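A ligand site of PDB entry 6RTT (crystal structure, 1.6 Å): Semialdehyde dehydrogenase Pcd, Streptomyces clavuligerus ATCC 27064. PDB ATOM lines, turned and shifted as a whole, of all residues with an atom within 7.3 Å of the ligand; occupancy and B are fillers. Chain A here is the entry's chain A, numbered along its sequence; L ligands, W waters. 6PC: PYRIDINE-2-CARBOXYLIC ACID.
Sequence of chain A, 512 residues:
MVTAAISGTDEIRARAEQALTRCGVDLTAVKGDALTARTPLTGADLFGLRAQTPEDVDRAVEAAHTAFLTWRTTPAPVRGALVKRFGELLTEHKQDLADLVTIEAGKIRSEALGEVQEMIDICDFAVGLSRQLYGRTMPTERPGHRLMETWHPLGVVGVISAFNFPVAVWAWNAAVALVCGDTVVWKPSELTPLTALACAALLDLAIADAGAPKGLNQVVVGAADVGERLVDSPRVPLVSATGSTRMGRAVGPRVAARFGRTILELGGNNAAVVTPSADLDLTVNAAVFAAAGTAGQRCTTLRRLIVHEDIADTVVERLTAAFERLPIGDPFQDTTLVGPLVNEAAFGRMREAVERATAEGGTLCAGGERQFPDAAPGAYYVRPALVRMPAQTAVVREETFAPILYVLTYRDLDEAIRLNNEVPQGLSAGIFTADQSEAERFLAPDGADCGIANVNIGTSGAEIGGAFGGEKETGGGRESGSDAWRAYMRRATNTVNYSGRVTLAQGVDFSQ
Water W1 lies within hydrogen-bond range of O1 of the ligand (2.8 Å) and O of Ser 460 (3.1 Å).
Water W2 bridges a nitrogen (N2) of the ligand (2.9 Å) and the side-chain carboxylate (OE1) of Glu 118 (3.0 Å).
The side-chain hydroxyl (OG) of Ser 460 sits at hydrogen-bond distance from the side-chain hydroxyl (OG1) of Thr 300 (2.7 Å).
The backbone carbonyl oxygen (O) of Thr 300 lies within hydrogen-bond range of the side-chain hydroxyl (OG1) of Thr 459 (2.8 Å).
The side-chain amide nitrogen of Asn 270 lies close to the backbone carbonyl oxygen of Thr 300 (3.4 Å).
O of Cys 299 is in hydrogen-bond range of ND2 of Asn 270, at 2.9 Å.
NE1 of Trp 172 lies within hydrogen-bond range of OE2 of Glu 118.
The side-chain hydroxyl (OG) of Ser 460 is in hydrogen-bond range of the guanidinium group (NH1) of Arg 298, 2.9 Å away.
The side-chain hydroxyl of Thr 301 is in hydrogen-bond range of the backbone NH of Arg 298 (2.9 Å).
The backbone carbonyl oxygen (O) of Phe 468 sits at hydrogen-bond distance from the backbone NH (N) of Glu 479.
OE1 of Glu 118 touches C3 of the ligand, at 3.7 Å.
Phe 165 touches the ligand (CE1 to C1, 3.4 Å).
Val 169 touches the ligand (CG2 to C5, 3.6 Å).
CH2 of Trp 172 touches C4 of the ligand, at 3.2 Å.
Arg 298 touches the ligand (CB to O2, 3.6 Å).
Phe 468 touches the ligand (CZ to C6, 3.9 Å).
The nearest printed residue that does not touch the ligand is Ser 460 (4.4 Å).
An oxygen (O2) of the ligand is in hydrogen-bond range of the backbone NH of Thr 300, 3.0 Å away.
O1 of the ligand lies within hydrogen-bond range of OG1 of Thr 300 (2.6 Å).
The backbone NH of Cys 299 lies within hydrogen-bond range of an oxygen (O2) of the ligand (2.9 Å).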
ATOM      1  N   LYS A 107      27.333 -32.398 -22.564  1.00  0.00           N
ATOM      2  CA  LYS A 107      25.939 -32.148 -22.241  1.00  0.00           C
ATOM      3  C   LYS A 107      25.076 -33.311 -22.715  1.00  0.00           C
ATOM      4  O   LYS A 107      25.438 -34.062 -23.628  1.00  0.00           O
ATOM      5  CB  LYS A 107      25.462 -30.827 -22.856  1.00  0.00           C
ATOM      6  CG  LYS A 107      25.514 -30.769 -24.357  1.00  0.00           C
ATOM      7  CD  LYS A 107      24.941 -29.417 -24.851  1.00  0.00           C
ATOM      8  CE  LYS A 107      25.869 -28.245 -24.533  1.00  0.00           C
ATOM      9  NZ  LYS A 107      25.243 -26.924 -24.902  1.00  0.00           N
ATOM     10  N   GLU A 115      20.752 -27.816 -29.058  1.00  0.00           N
ATOM     11  CA  GLU A 115      21.717 -26.817 -29.506  1.00  0.00           C
ATOM     12  C   GLU A 115      21.871 -26.835 -31.027  1.00  0.00           C
ATOM     13  O   GLU A 115      21.975 -25.781 -31.669  1.00  0.00           O
ATOM     14  CB  GLU A 115      23.077 -27.029 -28.832  1.00  0.00           C
ATOM     15  CG  GLU A 115      24.051 -25.929 -29.227  1.00  0.00           C
ATOM     16  CD  GLU A 115      25.410 -26.004 -28.549  1.00  0.00           C
ATOM     17  OE1 GLU A 115      25.610 -26.828 -27.630  1.00  0.00           O
ATOM     18  OE2 GLU A 115      26.299 -25.216 -28.971  1.00  0.00           O
ATOM     19  N   GLU A 118      18.997 -25.062 -32.433  1.00  0.00           N
ATOM     20  CA  GLU A 118      19.203 -23.611 -32.382  1.00  0.00           C
ATOM     21  C   GLU A 118      19.899 -23.123 -33.653  1.00  0.00           C
ATOM     22  O   GLU A 118      19.554 -22.061 -34.183  1.00  0.00           O
ATOM     23  CB  GLU A 118      20.058 -23.223 -31.175  1.00  0.00           C
ATOM     24  CG  GLU A 118      19.323 -23.076 -29.866  1.00  0.00           C
ATOM     25  CD  GLU A 118      20.175 -22.336 -28.840  1.00  0.00           C
ATOM     26  OE1 GLU A 118      20.440 -22.899 -27.758  1.00  0.00           O
ATOM     27  OE2 GLU A 118      20.579 -21.182 -29.142  1.00  0.00           O
ATOM     28  N   ASN A 164      31.098 -24.520 -23.936  1.00  0.00           N
ATOM     29  CA  ASN A 164      29.833 -24.987 -23.382  1.00  0.00           C
ATOM     30  C   ASN A 164      28.702 -24.936 -24.389  1.00  0.00           C
ATOM     31  O   ASN A 164      27.763 -25.743 -24.296  1.00  0.00           O
ATOM     32  CB  ASN A 164      29.471 -24.213 -22.110  1.00  0.00           C
ATOM     33  CG  ASN A 164      29.318 -22.721 -22.333  1.00  0.00           C
ATOM     34  OD1 ASN A 164      29.964 -22.127 -23.199  1.00  0.00           O
ATOM     35  ND2 ASN A 164      28.448 -22.101 -21.537  1.00  0.00           N
ATOM     36  N   PHE A 165      28.768 -24.037 -25.365  1.00  0.00           N
ATOM     37  CA  PHE A 165      27.854 -24.020 -26.501  1.00  0.00           C
ATOM     38  C   PHE A 165      28.732 -24.003 -27.735  1.00  0.00           C
ATOM     39  O   PHE A 165      28.949 -22.945 -28.349  1.00  0.00           O
ATOM     40  CB  PHE A 165      26.879 -22.852 -26.412  1.00  0.00           C
ATOM     41  CG  PHE A 165      25.799 -23.080 -25.411  1.00  0.00           C
ATOM     42  CD1 PHE A 165      26.001 -22.735 -24.079  1.00  0.00           C
ATOM     43  CD2 PHE A 165      24.629 -23.723 -25.772  1.00  0.00           C
ATOM     44  CE1 PHE A 165      25.022 -22.983 -23.133  1.00  0.00           C
ATOM     45  CE2 PHE A 165      23.648 -23.969 -24.835  1.00  0.00           C
ATOM     46  CZ  PHE A 165      23.845 -23.599 -23.515  1.00  0.00           C
ATOM     47  N   ALA A 168      26.183 -23.487 -31.208  1.00  0.00           N
ATOM     48  CA  ALA A 168      25.093 -22.506 -31.356  1.00  0.00           C
ATOM     49  C   ALA A 168      25.617 -21.085 -31.437  1.00  0.00           C
ATOM     50  O   ALA A 168      25.096 -20.271 -32.204  1.00  0.00           O
ATOM     51  CB  ALA A 168      24.091 -22.625 -30.213  1.00  0.00           C
ATOM     52  N   VAL A 169      26.624 -20.738 -30.629  1.00  0.00           N
ATOM     53  CA  VAL A 169      27.122 -19.360 -30.625  1.00  0.00           C
ATOM     54  C   VAL A 169      27.732 -19.017 -31.975  1.00  0.00           C
ATOM     55  O   VAL A 169      27.474 -17.943 -32.535  1.00  0.00           O
ATOM     56  CB  VAL A 169      28.124 -19.159 -29.471  1.00  0.00           C
ATOM     57  CG1 VAL A 169      28.873 -17.850 -29.634  1.00  0.00           C
ATOM     58  CG2 VAL A 169      27.401 -19.190 -28.138  1.00  0.00           C
ATOM     59  N   TRP A 172      24.852 -18.505 -34.441  1.00  0.00           N
ATOM     60  CA  TRP A 172      24.252 -17.178 -34.301  1.00  0.00           C
ATOM     61  C   TRP A 172      25.061 -16.153 -35.058  1.00  0.00           C
ATOM     62  O   TRP A 172      24.522 -15.324 -35.786  1.00  0.00           O
ATOM     63  CB  TRP A 172      24.204 -16.728 -32.844  1.00  0.00           C
ATOM     64  CG  TRP A 172      23.288 -17.428 -31.898  1.00  0.00           C
ATOM     65  CD1 TRP A 172      22.285 -18.309 -32.193  1.00  0.00           C
ATOM     66  CD2 TRP A 172      23.320 -17.298 -30.475  1.00  0.00           C
ATOM     67  NE1 TRP A 172      21.679 -18.719 -31.015  1.00  0.00           N
ATOM     68  CE2 TRP A 172      22.313 -18.123 -29.962  1.00  0.00           C
ATOM     69  CE3 TRP A 172      24.118 -16.557 -29.589  1.00  0.00           C
ATOM     70  CZ2 TRP A 172      22.050 -18.216 -28.590  1.00  0.00           C
ATOM     71  CZ3 TRP A 172      23.865 -16.655 -28.231  1.00  0.00           C
ATOM     72  CH2 TRP A 172      22.844 -17.482 -27.749  1.00  0.00           C
ATOM     73  N   THR A 242      32.716 -14.911 -26.751  1.00  0.00           N
ATOM     74  CA  THR A 242      31.950 -15.518 -25.679  1.00  0.00           C
ATOM     75  C   THR A 242      32.914 -16.317 -24.823  1.00  0.00           C
ATOM     76  O   THR A 242      33.757 -17.049 -25.343  1.00  0.00           O
ATOM     77  CB  THR A 242      30.831 -16.413 -26.249  1.00  0.00           C
ATOM     78  OG1 THR A 242      29.962 -15.615 -27.066  1.00  0.00           O
ATOM     79  CG2 THR A 242      30.004 -17.056 -25.127  1.00  0.00           C
ATOM     80  N   GLU A 265      29.926 -11.339 -24.701  1.00  0.00           N
ATOM     81  CA  GLU A 265      28.980 -12.026 -23.831  1.00  0.00           C
ATOM     82  C   GLU A 265      29.813 -12.930 -22.938  1.00  0.00           C
ATOM     83  O   GLU A 265      30.264 -14.006 -23.355  1.00  0.00           O
ATOM     84  CB  GLU A 265      27.961 -12.807 -24.655  1.00  0.00           C
ATOM     85  CG  GLU A 265      26.744 -13.232 -23.838  1.00  0.00           C
ATOM     86  CD  GLU A 265      27.007 -14.493 -23.022  1.00  0.00           C
ATOM     87  OE1 GLU A 265      27.007 -15.593 -23.625  1.00  0.00           O
ATOM     88  OE2 GLU A 265      27.215 -14.375 -21.799  1.00  0.00           O
ATOM     89  N   GLY A 267      29.207 -14.312 -19.774  1.00  0.00           N
ATOM     90  CA  GLY A 267      28.612 -15.118 -18.741  1.00  0.00           C
ATOM     91  C   GLY A 267      27.833 -14.307 -17.725  1.00  0.00           C
ATOM     92  O   GLY A 267      27.748 -13.077 -17.790  1.00  0.00           O
ATOM     93  N   ASN A 270      23.553 -15.503 -12.418  1.00  0.00           N
ATOM     94  CA  ASN A 270      22.142 -15.180 -12.578  1.00  0.00           C
ATOM     95  C   ASN A 270      21.307 -15.605 -11.382  1.00  0.00           C
ATOM     96  O   ASN A 270      21.487 -16.698 -10.827  1.00  0.00           O
ATOM     97  CB  ASN A 270      21.631 -15.842 -13.853  1.00  0.00           C
ATOM     98  CG  ASN A 270      22.615 -15.672 -14.997  1.00  0.00           C
ATOM     99  OD1 ASN A 270      22.836 -14.558 -15.466  1.00  0.00           O
ATOM    100  ND2 ASN A 270      23.294 -16.754 -15.376  1.00  0.00           N
ATOM    101  N   THR A 294      23.034 -28.794 -17.690  1.00  0.00           N
ATOM    102  CA  THR A 294      24.361 -28.604 -18.282  1.00  0.00           C
ATOM    103  C   THR A 294      25.439 -28.594 -17.193  1.00  0.00           C
ATOM    104  O   THR A 294      26.493 -27.979 -17.368  1.00  0.00           O
ATOM    105  CB  THR A 294      24.409 -27.325 -19.128  1.00  0.00           C
ATOM    106  OG1 THR A 294      23.157 -27.147 -19.787  1.00  0.00           O
ATOM    107  CG2 THR A 294      25.499 -27.399 -20.210  1.00  0.00           C
ATOM    108  N   GLN A 297      26.967 -25.260 -16.272  1.00  0.00           N
ATOM    109  CA  GLN A 297      27.946 -24.679 -17.192  1.00  0.00           C
ATOM    110  C   GLN A 297      27.278 -23.939 -18.346  1.00  0.00           C
ATOM    111  O   GLN A 297      27.781 -23.934 -19.474  1.00  0.00           O
ATOM    112  CB  GLN A 297      28.895 -25.756 -17.727  1.00  0.00           C
ATOM    113  CG  GLN A 297      29.684 -26.468 -16.634  1.00  0.00           C
ATOM    114  CD  GLN A 297      30.557 -27.583 -17.181  1.00  0.00           C
ATOM    115  OE1 GLN A 297      31.738 -27.664 -16.883  1.00  0.00           O
ATOM    116  NE2 GLN A 297      29.963 -28.465 -17.985  1.00  0.00           N
ATOM    117  N   ARG A 298      26.133 -23.315 -18.084  1.00  0.00           N
ATOM    118  CA  ARG A 298      25.544 -22.364 -19.019  1.00  0.00           C
ATOM    119  C   ARG A 298      25.909 -20.942 -18.618  1.00  0.00           C
ATOM    120  O   ARG A 298      26.054 -20.639 -17.430  1.00  0.00           O
ATOM    121  CB  ARG A 298      24.017 -22.456 -19.078  1.00  0.00           C
ATOM    122  CG  ARG A 298      23.426 -23.826 -19.289  1.00  0.00           C
ATOM    123  CD  ARG A 298      21.906 -23.727 -19.157  1.00  0.00           C
ATOM    124  NE  ARG A 298      21.274 -25.049 -19.187  1.00  0.00           N
ATOM    125  CZ  ARG A 298      20.059 -25.324 -18.735  1.00  0.00           C
ATOM    126  NH1 ARG A 298      19.311 -24.358 -18.204  1.00  0.00           N
ATOM    127  NH2 ARG A 298      19.592 -26.564 -18.815  1.00  0.00           N
ATOM    128  N   CYS A 299      26.082 -20.076 -19.611  1.00  0.00           N
ATOM    129  CA  CYS A 299      26.176 -18.660 -19.289  1.00  0.00           C
ATOM    130  C   CYS A 299      24.955 -18.202 -18.495  1.00  0.00           C
ATOM    131  O   CYS A 299      25.074 -17.350 -17.598  1.00  0.00           O
ATOM    132  CB  CYS A 299      26.308 -17.837 -20.566  1.00  0.00           C
ATOM    133  SG  CYS A 299      27.885 -18.111 -21.479  1.00  0.00           S
ATOM    134  N   THR A 300      23.796 -18.800 -18.768  1.00  0.00           N
ATOM    135  CA  THR A 300      22.536 -18.435 -18.117  1.00  0.00           C
ATOM    136  C   THR A 300      22.209 -19.276 -16.890  1.00  0.00           C
ATOM    137  O   THR A 300      21.083 -19.194 -16.386  1.00  0.00           O
ATOM    138  CB  THR A 300      21.376 -18.575 -19.109  1.00  0.00           C
ATOM    139  OG1 THR A 300      21.283 -19.941 -19.542  1.00  0.00           O
ATOM    140  CG2 THR A 300      21.572 -17.657 -20.300  1.00  0.00           C
ATOM    141  N   THR A 301      23.150 -20.078 -16.394  1.00  0.00           N
ATOM    142  CA  THR A 301      22.872 -20.957 -15.252  1.00  0.00           C
ATOM    143  C   THR A 301      22.378 -20.158 -14.037  1.00  0.00           C
ATOM    144  O   THR A 301      22.884 -19.083 -13.720  1.00  0.00           O
ATOM    145  CB  THR A 301      24.146 -21.748 -14.876  1.00  0.00           C
ATOM    146  OG1 THR A 301      24.390 -22.758 -15.858  1.00  0.00           O
ATOM    147  CG2 THR A 301      23.996 -22.406 -13.498  1.00  0.00           C
ATOM    148  N   PHE A 401      32.001 -21.311 -12.397  1.00  0.00           N
ATOM    149  CA  PHE A 401      31.355 -21.991 -13.519  1.00  0.00           C
ATOM    150  C   PHE A 401      31.140 -23.461 -13.159  1.00  0.00           C
ATOM    151  O   PHE A 401      31.803 -24.377 -13.650  1.00  0.00           O
ATOM    152  CB  PHE A 401      32.164 -21.828 -14.799  1.00  0.00           C
ATOM    153  CG  PHE A 401      31.329 -21.732 -16.038  1.00  0.00           C
ATOM    154  CD1 PHE A 401      30.432 -20.698 -16.207  1.00  0.00           C
ATOM    155  CD2 PHE A 401      31.440 -22.686 -17.045  1.00  0.00           C
ATOM    156  CE1 PHE A 401      29.649 -20.602 -17.336  1.00  0.00           C
ATOM    157  CE2 PHE A 401      30.656 -22.596 -18.187  1.00  0.00           C
ATOM    158  CZ  PHE A 401      29.761 -21.559 -18.334  1.00  0.00           C
ATOM    159  N   LEU A 427      23.602 -10.856 -16.704  1.00  0.00           N
ATOM    160  CA  LEU A 427      23.080 -11.528 -17.895  1.00  0.00           C
ATOM    161  C   LEU A 427      21.566 -11.723 -17.778  1.00  0.00           C
ATOM    162  O   LEU A 427      20.803 -11.089 -18.517  1.00  0.00           O
ATOM    163  CB  LEU A 427      23.788 -12.877 -18.112  1.00  0.00           C
ATOM    164  CG  LEU A 427      23.290 -13.695 -19.303  1.00  0.00           C
ATOM    165  CD1 LEU A 427      23.217 -12.873 -20.593  1.00  0.00           C
ATOM    166  CD2 LEU A 427      24.218 -14.890 -19.512  1.00  0.00           C
ATOM    167  N   THR A 459      16.338 -18.482 -15.514  1.00  0.00           N
ATOM    168  CA  THR A 459      17.378 -17.628 -16.065  1.00  0.00           C
ATOM    169  C   THR A 459      17.862 -18.083 -17.440  1.00  0.00           C
ATOM    170  O   THR A 459      18.569 -17.310 -18.096  1.00  0.00           O
ATOM    171  CB  THR A 459      18.538 -17.558 -15.085  1.00  0.00           C
ATOM    172  OG1 THR A 459      18.904 -18.890 -14.692  1.00  0.00           O
ATOM    173  CG2 THR A 459      18.138 -16.764 -13.854  1.00  0.00           C
ATOM    174  N   SER A 460      17.532 -19.301 -17.863  1.00  0.00           N
ATOM    175  CA  SER A 460      17.836 -19.766 -19.215  1.00  0.00           C
ATOM    176  C   SER A 460      16.685 -19.508 -20.181  1.00  0.00           C
ATOM    177  O   SER A 460      16.754 -19.970 -21.326  1.00  0.00           O
ATOM    178  CB  SER A 460      18.183 -21.264 -19.204  1.00  0.00           C
ATOM    179  OG  SER A 460      19.364 -21.516 -18.453  1.00  0.00           O
ATOM    180  N   GLY A 461      15.645 -18.803 -19.747  1.00  0.00           N
ATOM    181  CA  GLY A 461      14.505 -18.488 -20.601  1.00  0.00           C
ATOM    182  C   GLY A 461      14.848 -17.446 -21.634  1.00  0.00           C
ATOM    183  O   GLY A 461      14.737 -16.245 -21.385  1.00  0.00           O
ATOM    184  N   ALA A 462      15.281 -17.906 -22.801  1.00  0.00           N
ATOM    185  CA  ALA A 462      15.615 -17.053 -23.939  1.00  0.00           C
ATOM    186  C   ALA A 462      15.384 -17.866 -25.199  1.00  0.00           C
ATOM    187  O   ALA A 462      15.303 -19.097 -25.163  1.00  0.00           O
ATOM    188  CB  ALA A 462      17.056 -16.544 -23.855  1.00  0.00           C
ATOM    189  N   PHE A 468      20.133 -11.660 -27.342  1.00  0.00           N
ATOM    190  CA  PHE A 468      20.744 -12.404 -26.256  1.00  0.00           C
ATOM    191  C   PHE A 468      22.028 -11.715 -25.801  1.00  0.00           C
ATOM    192  O   PHE A 468      22.930 -11.481 -26.613  1.00  0.00           O
ATOM    193  CB  PHE A 468      21.060 -13.839 -26.677  1.00  0.00           C
ATOM    194  CG  PHE A 468      21.638 -14.688 -25.578  1.00  0.00           C
ATOM    195  CD1 PHE A 468      23.010 -14.764 -25.404  1.00  0.00           C
ATOM    196  CD2 PHE A 468      20.819 -15.421 -24.743  1.00  0.00           C
ATOM    197  CE1 PHE A 468      23.558 -15.543 -24.394  1.00  0.00           C
ATOM    198  CE2 PHE A 468      21.358 -16.211 -23.735  1.00  0.00           C
ATOM    199  CZ  PHE A 468      22.728 -16.269 -23.554  1.00  0.00           C
ATOM    200  N   GLU A 479      23.409 -10.817 -29.338  1.00  0.00           N
ATOM    201  CA  GLU A 479      23.463 -11.736 -30.464  1.00  0.00           C
ATOM    202  C   GLU A 479      22.079 -12.281 -30.759  1.00  0.00           C
ATOM    203  O   GLU A 479      21.134 -12.098 -29.993  1.00  0.00           O
ATOM    204  CB  GLU A 479      24.424 -12.909 -30.180  1.00  0.00           C
ATOM    205  CG  GLU A 479      25.823 -12.465 -29.899  1.00  0.00           C
ATOM    206  CD  GLU A 479      26.631 -13.544 -29.241  1.00  0.00           C
ATOM    207  OE1 GLU A 479      27.512 -14.098 -29.920  1.00  0.00           O
ATOM    208  OE2 GLU A 479      26.355 -13.850 -28.056  1.00  0.00           O
HETATM  209  C1  6PC L   1      23.382 -20.128 -23.827  1.00  0.00           C
HETATM  210  C3  6PC L   1      22.874 -20.612 -26.054  1.00  0.00           C
HETATM  211  C4  6PC L   1      24.094 -20.075 -26.429  1.00  0.00           C
HETATM  212  C2  6PC L   1      22.999 -20.174 -22.358  1.00  0.00           C
HETATM  213  C5  6PC L   1      24.942 -19.564 -25.511  1.00  0.00           C
HETATM  214  C6  6PC L   1      24.592 -19.593 -24.201  1.00  0.00           C
HETATM  215  O1  6PC L   1      21.820 -20.483 -22.009  1.00  0.00           O
HETATM  216  O2  6PC L   1      23.875 -19.878 -21.516  1.00  0.00           O
HETATM  217  N2  6PC L   1      22.521 -20.628 -24.750  1.00  0.00           N
HETATM  218  O   HOH W   1      19.332 -19.459 -22.882  1.00  0.00           O
HETATM  219  O   HOH W   2      20.086 -22.275 -24.822  1.00  0.00           O
